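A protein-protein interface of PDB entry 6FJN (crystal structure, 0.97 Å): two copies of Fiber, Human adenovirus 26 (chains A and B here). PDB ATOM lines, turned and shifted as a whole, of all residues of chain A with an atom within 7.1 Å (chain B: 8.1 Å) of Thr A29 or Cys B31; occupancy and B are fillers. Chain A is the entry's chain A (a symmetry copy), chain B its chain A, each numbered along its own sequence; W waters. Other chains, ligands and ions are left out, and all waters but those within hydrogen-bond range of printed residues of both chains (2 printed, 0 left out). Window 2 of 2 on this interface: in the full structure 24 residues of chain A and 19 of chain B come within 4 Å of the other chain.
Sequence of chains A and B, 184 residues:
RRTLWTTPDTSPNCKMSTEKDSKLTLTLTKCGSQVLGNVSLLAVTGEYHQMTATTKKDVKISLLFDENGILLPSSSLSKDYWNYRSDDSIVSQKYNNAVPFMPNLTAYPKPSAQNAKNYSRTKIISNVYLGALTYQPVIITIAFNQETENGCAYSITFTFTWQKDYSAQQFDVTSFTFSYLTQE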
ATOM      1  N   ARG A   1      12.227  23.619   1.363  1.00  0.00           N
ATOM      2  CA  ARG A   1      13.430  23.153   2.122  1.00  0.00           C
ATOM      3  C   ARG A   1      14.068  24.272   2.958  1.00  0.00           C
ATOM      4  O   ARG A   1      14.000  25.457   2.626  1.00  0.00           O
ATOM      5  CB  ARG A   1      14.407  22.406   1.213  1.00  0.00           C
ATOM      6  CG  ARG A   1      15.295  21.386   1.936  1.00  0.00           C
ATOM      7  CD  ARG A   1      16.715  21.914   2.199  1.00  0.00           C
ATOM      8  NE  ARG A   1      17.211  21.744   3.572  1.00  0.00           N
ATOM      9  CZ  ARG A   1      17.275  20.615   4.279  1.00  0.00           C
ATOM     10  NH1 ARG A   1      16.954  19.440   3.758  1.00  0.00           N
ATOM     11  NH2 ARG A   1      17.754  20.670   5.528  1.00  0.00           N
ATOM     12  N   ARG A   2      14.611  23.862   4.100  1.00  0.00           N
ATOM     13  CA  ARG A   2      14.912  24.757   5.207  1.00  0.00           C
ATOM     14  C   ARG A   2      16.371  25.052   5.425  1.00  0.00           C
ATOM     15  O   ARG A   2      16.637  25.858   6.272  1.00  0.00           O
ATOM     16  CB  ARG A   2      14.306  24.272   6.537  1.00  0.00           C
ATOM     17  CG  ARG A   2      12.852  24.688   6.820  1.00  0.00           C
ATOM     18  CD  ARG A   2      12.054  25.070   5.572  1.00  0.00           C
ATOM     19  NE  ARG A   2      11.636  26.482   5.512  1.00  0.00           N
ATOM     20  CZ  ARG A   2      10.908  26.987   4.510  1.00  0.00           C
ATOM     21  NH1 ARG A   2      10.530  28.266   4.490  1.00  0.00           N
ATOM     22  NH2 ARG A   2      10.546  26.203   3.513  1.00  0.00           N
ATOM     23  N   THR A   3      17.301  24.502   4.647  1.00  0.00           N
ATOM     24  CA  THR A   3      18.713  24.894   4.752  1.00  0.00           C
ATOM     25  C   THR A   3      19.275  25.211   3.370  1.00  0.00           C
ATOM     26  O   THR A   3      19.163  24.427   2.418  1.00  0.00           O
ATOM     27  CB  THR A   3      19.588  23.890   5.564  1.00  0.00           C
ATOM     28  OG1 THR A   3      19.281  24.010   6.994  1.00  0.00           O
ATOM     29  CG2 THR A   3      21.030  24.136   5.359  1.00  0.00           C
ATOM     30  N   LEU A   4      19.914  26.363   3.244  1.00  0.00           N
ATOM     31  CA  LEU A   4      20.761  26.711   2.094  1.00  0.00           C
ATOM     32  C   LEU A   4      22.194  26.629   2.564  1.00  0.00           C
ATOM     33  O   LEU A   4      22.526  27.157   3.661  1.00  0.00           O
ATOM     34  CB  LEU A   4      20.548  28.125   1.652  1.00  0.00           C
ATOM     35  CG  LEU A   4      19.396  28.606   0.853  1.00  0.00           C
ATOM     36  CD1 LEU A   4      19.593  30.091   0.542  1.00  0.00           C
ATOM     37  CD2 LEU A   4      19.359  27.807  -0.422  1.00  0.00           C
ATOM     38  N   THR A  27      26.211  27.988   6.201  1.00  0.00           N
ATOM     39  CA  THR A  27      24.945  27.300   6.320  1.00  0.00           C
ATOM     40  C   THR A  27      23.919  28.278   6.839  1.00  0.00           C
ATOM     41  O   THR A  27      24.159  28.943   7.866  1.00  0.00           O
ATOM     42  CB  THR A  27      25.097  26.126   7.310  1.00  0.00           C
ATOM     43  OG1 THR A  27      26.158  25.267   6.891  1.00  0.00           O
ATOM     44  CG2 THR A  27      23.844  25.279   7.423  1.00  0.00           C
ATOM     45  N   LEU A  28      22.789  28.369   6.142  1.00  0.00           N
ATOM     46  CA  LEU A  28      21.686  29.238   6.516  1.00  0.00           C
ATOM     47  C   LEU A  28      20.483  28.333   6.758  1.00  0.00           C
ATOM     48  O   LEU A  28      19.979  27.692   5.815  1.00  0.00           O
ATOM     49  CB  LEU A  28      21.398  30.231   5.400  1.00  0.00           C
ATOM     50  CG  LEU A  28      22.519  31.147   4.974  1.00  0.00           C
ATOM     51  CD1 LEU A  28      22.064  32.026   3.818  1.00  0.00           C
ATOM     52  CD2 LEU A  28      23.064  31.976   6.114  1.00  0.00           C
ATOM     53  N   THR A  29      20.018  28.262   8.015  1.00  0.00           N
ATOM     54  CA  THR A  29      18.903  27.411   8.368  1.00  0.00           C
ATOM     55  C   THR A  29      17.703  28.277   8.733  1.00  0.00           C
ATOM     56  O   THR A  29      17.802  29.128   9.643  1.00  0.00           O
ATOM     57  CB  THR A  29      19.264  26.496   9.533  1.00  0.00           C
ATOM     58  OG1 THR A  29      20.375  25.657   9.142  1.00  0.00           O
ATOM     59  CG2 THR A  29      18.049  25.660   9.942  1.00  0.00           C
ATOM     60  N   LYS A  30      16.614  28.104   8.030  1.00  0.00           N
ATOM     61  CA  LYS A  30      15.418  28.883   8.262  1.00  0.00           C
ATOM     62  C   LYS A  30      14.751  28.434   9.555  1.00  0.00           C
ATOM     63  O   LYS A  30      14.349  27.275   9.706  1.00  0.00           O
ATOM     64  CB  LYS A  30      14.502  28.671   7.067  1.00  0.00           C
ATOM     65  CG  LYS A  30      13.132  29.246   7.085  1.00  0.00           C
ATOM     66  CD  LYS A  30      13.203  30.724   7.126  1.00  0.00           C
ATOM     67  CE  LYS A  30      11.835  31.269   6.646  1.00  0.00           C
ATOM     68  NZ  LYS A  30      11.790  32.745   6.706  1.00  0.00           N
ATOM     69  N   CYS A  31      14.579  29.401  10.482  1.00  0.00           N
ATOM     70  CA  CYS A  31      13.872  29.247  11.719  1.00  0.00           C
ATOM     71  C   CYS A  31      12.729  30.289  11.782  1.00  0.00           C
ATOM     72  O   CYS A  31      12.865  31.314  12.487  1.00  0.00           O
ATOM     73  CB  CYS A  31      14.809  29.410  12.905  1.00  0.00           C
ATOM     74  SG  CYS A  31      16.177  28.228  12.946  1.00  0.00           S
ATOM     75  N   GLY A  32      11.727  30.151  10.954  1.00  0.00           N
ATOM     76  CA  GLY A  32      10.651  31.094  10.960  1.00  0.00           C
ATOM     77  C   GLY A  32      11.094  32.444  10.513  1.00  0.00           C
ATOM     78  O   GLY A  32      11.664  32.598   9.428  1.00  0.00           O
ATOM     79  N   GLN A  34      13.529  34.175  11.494  1.00  0.00           N
ATOM     80  CA  GLN A  34      14.997  34.344  11.467  1.00  0.00           C
ATOM     81  C   GLN A  34      15.670  33.224  10.704  1.00  0.00           C
ATOM     82  O   GLN A  34      15.128  32.118  10.644  1.00  0.00           O
ATOM     83  CB  GLN A  34      15.600  34.408  12.874  1.00  0.00           C
ATOM     84  CG  GLN A  34      15.167  35.646  13.637  1.00  0.00           C
ATOM     85  CD  GLN A  34      15.782  35.629  15.050  1.00  0.00           C
ATOM     86  OE1 GLN A  34      16.986  35.751  15.244  1.00  0.00           O
ATOM     87  NE2 GLN A  34      14.942  35.458  16.035  1.00  0.00           N
ATOM     88  N   VAL A  35      16.813  33.513  10.137  1.00  0.00           N
ATOM     89  CA  VAL A  35      17.760  32.500   9.718  1.00  0.00           C
ATOM     90  C   VAL A  35      18.811  32.360  10.816  1.00  0.00           C
ATOM     91  O   VAL A  35      19.313  33.363  11.346  1.00  0.00           O
ATOM     92  CB  VAL A  35      18.401  32.870   8.388  1.00  0.00           C
ATOM     93  CG1 VAL A  35      19.725  32.177   8.184  1.00  0.00           C
ATOM     94  CG2 VAL A  35      17.463  32.526   7.265  1.00  0.00           C
ATOM     95  N   LEU A  36      19.167  31.097  11.147  1.00  0.00           N
ATOM     96  CA  LEU A  36      20.294  30.757  11.958  1.00  0.00           C
ATOM     97  C   LEU A  36      21.455  30.465  11.024  1.00  0.00           C
ATOM     98  O   LEU A  36      21.381  29.500  10.228  1.00  0.00           O
ATOM     99  CB  LEU A  36      19.947  29.528  12.815  1.00  0.00           C
ATOM    100  CG  LEU A  36      21.020  29.026  13.753  1.00  0.00           C
ATOM    101  CD1 LEU A  36      21.390  30.042  14.806  1.00  0.00           C
ATOM    102  CD2 LEU A  36      20.592  27.712  14.386  1.00  0.00           C
ATOM    103  N   GLY A  37      22.471  31.294  11.080  1.00  0.00           N
ATOM    104  CA  GLY A  37      23.601  31.162  10.198  1.00  0.00           C
ATOM    105  C   GLY A  37      24.857  30.664  10.903  1.00  0.00           C
ATOM    106  O   GLY A  37      25.048  30.894  12.113  1.00  0.00           O
ATOM    107  N   ASN A  38      25.746  30.050  10.119  1.00  0.00           N
ATOM    108  CA  ASN A  38      27.003  29.521  10.657  1.00  0.00           C
ATOM    109  C   ASN A  38      28.033  29.692   9.549  1.00  0.00           C
ATOM    110  O   ASN A  38      27.789  29.206   8.410  1.00  0.00           O
ATOM    111  CB  ASN A  38      26.774  28.081  11.035  1.00  0.00           C
ATOM    112  CG  ASN A  38      27.969  27.411  11.606  1.00  0.00           C
ATOM    113  OD1 ASN A  38      28.842  26.983  10.841  1.00  0.00           O
ATOM    114  ND2 ASN A  38      28.012  27.122  12.906  1.00  0.00           N
ATOM    115  N   PHE A 101      14.941  33.190   2.824  1.00  0.00           N
ATOM    116  CA  PHE A 101      16.290  33.228   3.432  1.00  0.00           C
ATOM    117  C   PHE A 101      16.918  34.584   3.319  1.00  0.00           C
ATOM    118  O   PHE A 101      18.007  34.783   3.838  1.00  0.00           O
ATOM    119  CB  PHE A 101      17.205  32.210   2.768  1.00  0.00           C
ATOM    120  CG  PHE A 101      16.815  30.787   3.028  1.00  0.00           C
ATOM    121  CD1 PHE A 101      15.786  30.185   2.347  1.00  0.00           C
ATOM    122  CD2 PHE A 101      17.470  30.041   4.004  1.00  0.00           C
ATOM    123  CE1 PHE A 101      15.412  28.874   2.608  1.00  0.00           C
ATOM    124  CE2 PHE A 101      17.097  28.745   4.249  1.00  0.00           C
ATOM    125  CZ  PHE A 101      16.097  28.175   3.563  1.00  0.00           C
ATOM    126  N   TYR A 180      19.603  36.494  11.619  1.00  0.00           N
ATOM    127  CA  TYR A 180      19.039  37.724  11.078  1.00  0.00           C
ATOM    128  C   TYR A 180      17.615  37.536  10.740  1.00  0.00           C
ATOM    129  O   TYR A 180      17.133  36.422  10.503  1.00  0.00           O
ATOM    130  CB  TYR A 180      19.855  38.227   9.840  1.00  0.00           C
ATOM    131  CG  TYR A 180      19.900  37.216   8.696  1.00  0.00           C
ATOM    132  CD1 TYR A 180      18.928  37.263   7.676  1.00  0.00           C
ATOM    133  CD2 TYR A 180      20.893  36.278   8.595  1.00  0.00           C
ATOM    134  CE1 TYR A 180      18.983  36.388   6.619  1.00  0.00           C
ATOM    135  CE2 TYR A 180      20.956  35.389   7.522  1.00  0.00           C
ATOM    136  CZ  TYR A 180      19.997  35.458   6.532  1.00  0.00           C
ATOM    137  OH  TYR A 180      20.098  34.524   5.528  1.00  0.00           O
ATOM    138  N   THR A 182      14.348  37.706   8.474  1.00  0.00           N
ATOM    139  CA  THR A 182      14.145  37.391   7.059  1.00  0.00           C
ATOM    140  C   THR A 182      13.036  38.186   6.397  1.00  0.00           C
ATOM    141  O   THR A 182      12.059  38.656   7.042  1.00  0.00           O
ATOM    142  CB  THR A 182      13.852  35.915   6.879  1.00  0.00           C
ATOM    143  OG1 THR A 182      12.652  35.613   7.605  1.00  0.00           O
ATOM    144  CG2 THR A 182      14.936  34.994   7.406  1.00  0.00           C
ATOM    145  N   ARG B   2      13.186  16.806  20.040  1.00  0.00           N
ATOM    146  CA  ARG B   2      14.020  17.850  19.465  1.00  0.00           C
ATOM    147  C   ARG B   2      14.942  18.549  20.427  1.00  0.00           C
ATOM    148  O   ARG B   2      15.703  19.349  19.959  1.00  0.00           O
ATOM    149  CB  ARG B   2      13.197  18.914  18.715  1.00  0.00           C
ATOM    150  CG  ARG B   2      12.861  18.609  17.245  1.00  0.00           C
ATOM    151  CD  ARG B   2      12.931  17.125  16.878  1.00  0.00           C
ATOM    152  NE  ARG B   2      13.985  16.776  15.909  1.00  0.00           N
ATOM    153  CZ  ARG B   2      14.176  15.533  15.453  1.00  0.00           C
ATOM    154  NH1 ARG B   2      15.127  15.248  14.562  1.00  0.00           N
ATOM    155  NH2 ARG B   2      13.402  14.558  15.888  1.00  0.00           N
ATOM    156  N   THR B   3      14.958  18.219  21.717  1.00  0.00           N
ATOM    157  CA  THR B   3      15.953  18.786  22.637  1.00  0.00           C
ATOM    158  C   THR B   3      16.611  17.676  23.449  1.00  0.00           C
ATOM    159  O   THR B   3      15.950  16.832  24.069  1.00  0.00           O
ATOM    160  CB  THR B   3      15.407  19.957  23.512  1.00  0.00           C
ATOM    161  OG1 THR B   3      15.248  21.160  22.687  1.00  0.00           O
ATOM    162  CG2 THR B   3      16.314  20.263  24.638  1.00  0.00           C
ATOM    163  N   LEU B  28      20.794  21.195  23.813  1.00  0.00           N
ATOM    164  CA  LEU B  28      21.013  21.055  22.382  1.00  0.00           C
ATOM    165  C   LEU B  28      19.634  20.937  21.741  1.00  0.00           C
ATOM    166  O   LEU B  28      18.915  19.946  21.976  1.00  0.00           O
ATOM    167  CB  LEU B  28      21.848  19.816  22.097  1.00  0.00           C
ATOM    168  CG  LEU B  28      23.214  19.733  22.734  1.00  0.00           C
ATOM    169  CD1 LEU B  28      23.874  18.407  22.381  1.00  0.00           C
ATOM    170  CD2 LEU B  28      24.101  20.902  22.374  1.00  0.00           C
ATOM    171  N   THR B  29      19.248  21.942  20.940  1.00  0.00           N
ATOM    172  CA  THR B  29      17.948  21.953  20.305  1.00  0.00           C
ATOM    173  C   THR B  29      18.120  21.770  18.802  1.00  0.00           C
ATOM    174  O   THR B  29      18.838  22.563  18.155  1.00  0.00           O
ATOM    175  CB  THR B  29      17.211  23.256  20.596  1.00  0.00           C
ATOM    176  OG1 THR B  29      17.024  23.379  22.023  1.00  0.00           O
ATOM    177  CG2 THR B  29      15.874  23.281  19.852  1.00  0.00           C
ATOM    178  N   LYS B  30      17.520  20.743  18.259  1.00  0.00           N
ATOM    179  CA  LYS B  30      17.628  20.447  16.848  1.00  0.00           C
ATOM    180  C   LYS B  30      16.811  21.451  16.045  1.00  0.00           C
ATOM    181  O   LYS B  30      15.590  21.563  16.202  1.00  0.00           O
ATOM    182  CB  LYS B  30      17.116  19.030  16.642  1.00  0.00           C
ATOM    183  CG  LYS B  30      16.982  18.494  15.263  1.00  0.00           C
ATOM    184  CD  LYS B  30      18.313  18.409  14.621  1.00  0.00           C
ATOM    185  CE  LYS B  30      18.196  17.414  13.439  1.00  0.00           C
ATOM    186  NZ  LYS B  30      19.470  17.304  12.696  1.00  0.00           N
ATOM    187  N   CYS B  31      17.503  22.150  15.119  1.00  0.00           N
ATOM    188  CA  CYS B  31      16.933  23.057  14.168  1.00  0.00           C
ATOM    189  C   CYS B  31      17.311  22.598  12.739  1.00  0.00           C
ATOM    190  O   CYS B  31      18.217  23.196  12.117  1.00  0.00           O
ATOM    191  CB  CYS B  31      17.411  24.479  14.416  1.00  0.00           C
ATOM    192  SG  CYS B  31      17.005  25.130  16.054  1.00  0.00           S
ATOM    193  N   GLY B  32      16.794  21.482  12.296  1.00  0.00           N
ATOM    194  CA  GLY B  32      17.121  21.004  10.988  1.00  0.00           C
ATOM    195  C   GLY B  32      18.555  20.613  10.884  1.00  0.00           C
ATOM    196  O   GLY B  32      19.049  19.797  11.669  1.00  0.00           O
ATOM    197  N   SER B  33      19.291  21.236   9.966  1.00  0.00           N
ATOM    198  CA  SER B  33      20.694  20.927   9.696  1.00  0.00           C
ATOM    199  C   SER B  33      21.671  21.484  10.731  1.00  0.00           C
ATOM    200  O   SER B  33      22.921  21.301  10.654  1.00  0.00           O
ATOM    201  CB  SER B  33      20.987  21.509   8.320  1.00  0.00           C
ATOM    202  OG  SER B  33      22.359  21.483   7.987  1.00  0.00           O
ATOM    203  N   GLN B  34      21.131  22.226  11.691  1.00  0.00           N
ATOM    204  CA  GLN B  34      21.967  22.714  12.808  1.00  0.00           C
ATOM    205  C   GLN B  34      21.360  22.362  14.149  1.00  0.00           C
ATOM    206  O   GLN B  34      20.138  22.223  14.245  1.00  0.00           O
ATOM    207  CB  GLN B  34      22.184  24.229  12.752  1.00  0.00           C
ATOM    208  CG  GLN B  34      23.007  24.655  11.550  1.00  0.00           C
ATOM    209  CD  GLN B  34      23.158  26.188  11.539  1.00  0.00           C
ATOM    210  OE1 GLN B  34      23.810  26.791  12.384  1.00  0.00           O
ATOM    211  NE2 GLN B  34      22.532  26.816  10.580  1.00  0.00           N
ATOM    212  N   VAL B  35      22.195  22.220  15.145  1.00  0.00           N
ATOM    213  CA  VAL B  35      21.781  22.276  16.532  1.00  0.00           C
ATOM    214  C   VAL B  35      22.054  23.688  17.045  1.00  0.00           C
ATOM    215  O   VAL B  35      23.126  24.258  16.792  1.00  0.00           O
ATOM    216  CB  VAL B  35      22.519  21.237  17.364  1.00  0.00           C
ATOM    217  CG1 VAL B  35      22.544  21.596  18.829  1.00  0.00           C
ATOM    218  CG2 VAL B  35      21.874  19.892  17.175  1.00  0.00           C
ATOM    219  N   LEU B  36      21.080  24.251  17.796  1.00  0.00           N
ATOM    220  CA  LEU B  36      21.237  25.443  18.568  1.00  0.00           C
ATOM    221  C   LEU B  36      21.600  25.027  19.982  1.00  0.00           C
ATOM    222  O   LEU B  36      20.785  24.360  20.660  1.00  0.00           O
ATOM    223  CB  LEU B  36      19.920  26.238  18.544  1.00  0.00           C
ATOM    224  CG  LEU B  36      19.898  27.546  19.301  1.00  0.00           C
ATOM    225  CD1 LEU B  36      20.875  28.553  18.744  1.00  0.00           C
ATOM    226  CD2 LEU B  36      18.487  28.111  19.333  1.00  0.00           C
ATOM    227  N   GLY B  37      22.800  25.361  20.398  1.00  0.00           N
ATOM    228  CA  GLY B  37      23.286  24.965  21.693  1.00  0.00           C
ATOM    229  C   GLY B  37      23.373  26.123  22.681  1.00  0.00           C
ATOM    230  O   GLY B  37      23.561  27.289  22.287  1.00  0.00           O
ATOM    231  N   PRO B 100      21.009  12.527  14.948  1.00  0.00           N
ATOM    232  CA  PRO B 100      20.693  13.861  14.414  1.00  0.00           C
ATOM    233  C   PRO B 100      21.175  15.039  15.245  1.00  0.00           C
ATOM    234  O   PRO B 100      21.055  16.185  14.759  1.00  0.00           O
ATOM    235  CB  PRO B 100      19.180  13.852  14.285  1.00  0.00           C
ATOM    236  CG  PRO B 100      18.870  12.371  14.104  1.00  0.00           C
ATOM    237  CD  PRO B 100      19.792  11.715  15.107  1.00  0.00           C
ATOM    238  N   PHE B 101      21.662  14.797  16.452  1.00  0.00           N
ATOM    239  CA  PHE B 101      22.273  15.844  17.303  1.00  0.00           C
ATOM    240  C   PHE B 101      23.770  15.828  17.223  1.00  0.00           C
ATOM    241  O   PHE B 101      24.408  16.683  17.821  1.00  0.00           O
ATOM    242  CB  PHE B 101      21.860  15.662  18.755  1.00  0.00           C
ATOM    243  CG  PHE B 101      20.403  15.906  19.004  1.00  0.00           C
ATOM    244  CD1 PHE B 101      19.451  14.965  18.701  1.00  0.00           C
ATOM    245  CD2 PHE B 101      19.968  17.123  19.523  1.00  0.00           C
ATOM    246  CE1 PHE B 101      18.101  15.204  18.911  1.00  0.00           C
ATOM    247  CE2 PHE B 101      18.633  17.347  19.732  1.00  0.00           C
ATOM    248  CZ  PHE B 101      17.722  16.408  19.439  1.00  0.00           C
ATOM    249  N   SER B 179      26.011  27.263  17.556  1.00  0.00           N
ATOM    250  CA  SER B 179      25.367  26.266  16.726  1.00  0.00           C
ATOM    251  C   SER B 179      26.412  25.433  16.028  1.00  0.00           C
ATOM    252  O   SER B 179      27.612  25.808  15.996  1.00  0.00           O
ATOM    253  CB  SER B 179      24.424  26.880  15.691  1.00  0.00           C
ATOM    254  OG  SER B 179      25.143  27.484  14.625  1.00  0.00           O
ATOM    255  N   TYR B 180      25.995  24.299  15.476  1.00  0.00           N
ATOM    256  CA  TYR B 180      26.861  23.469  14.649  1.00  0.00           C
ATOM    257  C   TYR B 180      26.060  22.661  13.710  1.00  0.00           C
ATOM    258  O   TYR B 180      24.874  22.380  13.922  1.00  0.00           O
ATOM    259  CB  TYR B 180      27.790  22.565  15.527  1.00  0.00           C
ATOM    260  CG  TYR B 180      27.018  21.623  16.449  1.00  0.00           C
ATOM    261  CD1 TYR B 180      26.693  20.322  16.015  1.00  0.00           C
ATOM    262  CD2 TYR B 180      26.664  21.983  17.722  1.00  0.00           C
ATOM    263  CE1 TYR B 180      26.039  19.450  16.850  1.00  0.00           C
ATOM    264  CE2 TYR B 180      26.003  21.101  18.577  1.00  0.00           C
ATOM    265  CZ  TYR B 180      25.700  19.830  18.132  1.00  0.00           C
ATOM    266  OH  TYR B 180      25.011  19.030  19.012  1.00  0.00           O
ATOM    267  N   LEU B 181      26.717  22.247  12.625  1.00  0.00           N
ATOM    268  CA  LEU B 181      26.111  21.405  11.612  1.00  0.00           C
ATOM    269  C   LEU B 181      25.994  19.982  12.114  1.00  0.00           C
ATOM    270  O   LEU B 181      26.897  19.470  12.726  1.00  0.00           O
ATOM    271  CB  LEU B 181      26.958  21.415  10.336  1.00  0.00           C
ATOM    272  CG  LEU B 181      26.860  22.666   9.467  1.00  0.00           C
ATOM    273  CD1 LEU B 181      27.008  24.015  10.115  1.00  0.00           C
ATOM    274  CD2 LEU B 181      27.830  22.511   8.287  1.00  0.00           C
ATOM    275  N   THR B 182      24.879  19.364  11.819  1.00  0.00           N
ATOM    276  CA  THR B 182      24.628  18.010  12.318  1.00  0.00           C
ATOM    277  C   THR B 182      24.867  16.916  11.296  1.00  0.00           C
ATOM    278  O   THR B 182      24.770  17.114  10.054  1.00  0.00           O
ATOM    279  CB  THR B 182      23.207  17.887  12.830  1.00  0.00           C
ATOM    280  OG1 THR B 182      22.320  18.158  11.736  1.00  0.00           O
ATOM    281  CG2 THR B 182      22.857  18.861  13.940  1.00  0.00           C
ATOM    282  N   GLU B 184      23.198  13.184   9.966  1.00  0.00           N
ATOM    283  CA  GLU B 184      21.819  12.630   9.959  1.00  0.00           C
ATOM    284  C   GLU B 184      21.901  11.119   9.989  1.00  0.00           C
ATOM    285  O   GLU B 184      20.972  10.390  10.423  1.00  0.00           O
ATOM    286  CB  GLU B 184      21.008  13.141   8.741  1.00  0.00           C
ATOM    287  CG  GLU B 184      20.777  14.663   8.707  1.00  0.00           C
ATOM    288  CD  GLU B 184      20.190  15.212  10.002  1.00  0.00           C
ATOM    289  OE1 GLU B 184      19.167  14.641  10.473  1.00  0.00           O
ATOM    290  OE2 GLU B 184      20.797  16.147  10.593  1.00  0.00           O
ATOM    291  OXT GLU B 184      22.963  10.602   9.611  1.00  0.00           O
HETATM  292  O   HOH W   1      29.948  26.108  14.670  1.00  0.00           O
HETATM  293  O   HOH W   2      17.483  22.240   7.783  1.00  0.00           O
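OG1 of Thr A3 touches CB of Ser B33, at 3.3 Å.
Thr A27 touches Gln B34 (CG2 to NE2, 3.7 Å).
CD2 of Leu B181 touches OG1 of Thr A27 (3.5 Å).
O of Cys B31 touches CG2 of Thr A29 (3.3 Å).
OE1 of Gln B34 touches CB of Asn A38, 3.5 Å away.
OD1 of Asn A38 touches CD1 of Leu B181, at 3.6 Å.
Thr A29 touches Cys B31, but with the chains exchanged Cys A31 does not touch Thr B29 (8.1 Å).
Thr A29 touches Gln B34, but with the chains exchanged Gln A34 does not touch Thr B29 (12.7 Å).
Leu A36 touches Gln B34, but with the chains exchanged Gln A34 does not touch Leu B36 (8.8 Å).
The side-chain amide nitrogen (NE2) of Gln B34 sits at hydrogen-bond distance from the side-chain hydroxyl (OG1) of Thr A29 (2.8 Å).
O of Leu A36 is in hydrogen-bond range of NE2 of Gln B34, at 2.9 Å.
The side-chain amide nitrogen of Asn A38 lies within hydrogen-bond range of the side-chain hydroxyl of Ser B179 (3.4 Å).
Water W2 lies within hydrogen-bond range of OG1 of Thr A3 (2.6 Å), NH2 of Arg A1 (2.8 Å) and N of Ser B33 (3.0 Å).
Water W1 bridges the backbone carbonyl oxygen of Ser B179 (2.7 Å) and the side-chain amide nitrogen of Asn A38 (2.8 Å).
Of the printed residues of chain B, Thr A29 touches Cys B31 and Gln B34.
Of chain A, only Thr A29 (3.3 Å) comes within 4 Å of Cys B31.
Printed residues of chain A within 4 Å of Leu B181: Thr A27 (3.5 Å) and Asn A38 (3.6 Å).
Printed residues of chain B within 4 Å of Thr A3: Ser B33.
Printed residues of chain B within 4 Å of Thr A27: Gln B34 and Leu B181.
Printed residues of chain A within 4 Å of Ser B179: Asn A38.
The nearest printed residue of chain B that does not touch Thr A29 is Ser B33 (4.3 Å).
O of Thr B29 sits at hydrogen-bond distance from SG of Cys B31, at 3.8 Å.
The side-chain amide oxygen (OE1) of Gln B34 is in hydrogen-bond range of the side-chain hydroxyl (OG) of Ser B179, at 2.7 Å.
The side-chain hydroxyl (OG1) of Thr A3 lies within hydrogen-bond range of the side-chain hydroxyl (OG1) of Thr A29, 2.9 Å away.
The backbone carbonyl oxygen of Thr A27 lies within hydrogen-bond range of the backbone NH of Asn A38, at 3.0 Å.
The backbone carbonyl oxygen (O) of Thr A29 sits at hydrogen-bond distance from the side-chain sulfur (SG) of Cys A31.
The backbone carbonyl oxygen (O) of Thr A29 lies within hydrogen-bond range of the backbone NH (N) of Leu A36, at 2.8 Å.
Hydrophobic or aromatic side chains of chain A within 4 Å of the printed part of chain B: Leu A36.
Among the printed residues, no Asp or Glu carboxylate lies within 4 Å of a Lys or Arg side-chain nitrogen of the other chain.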
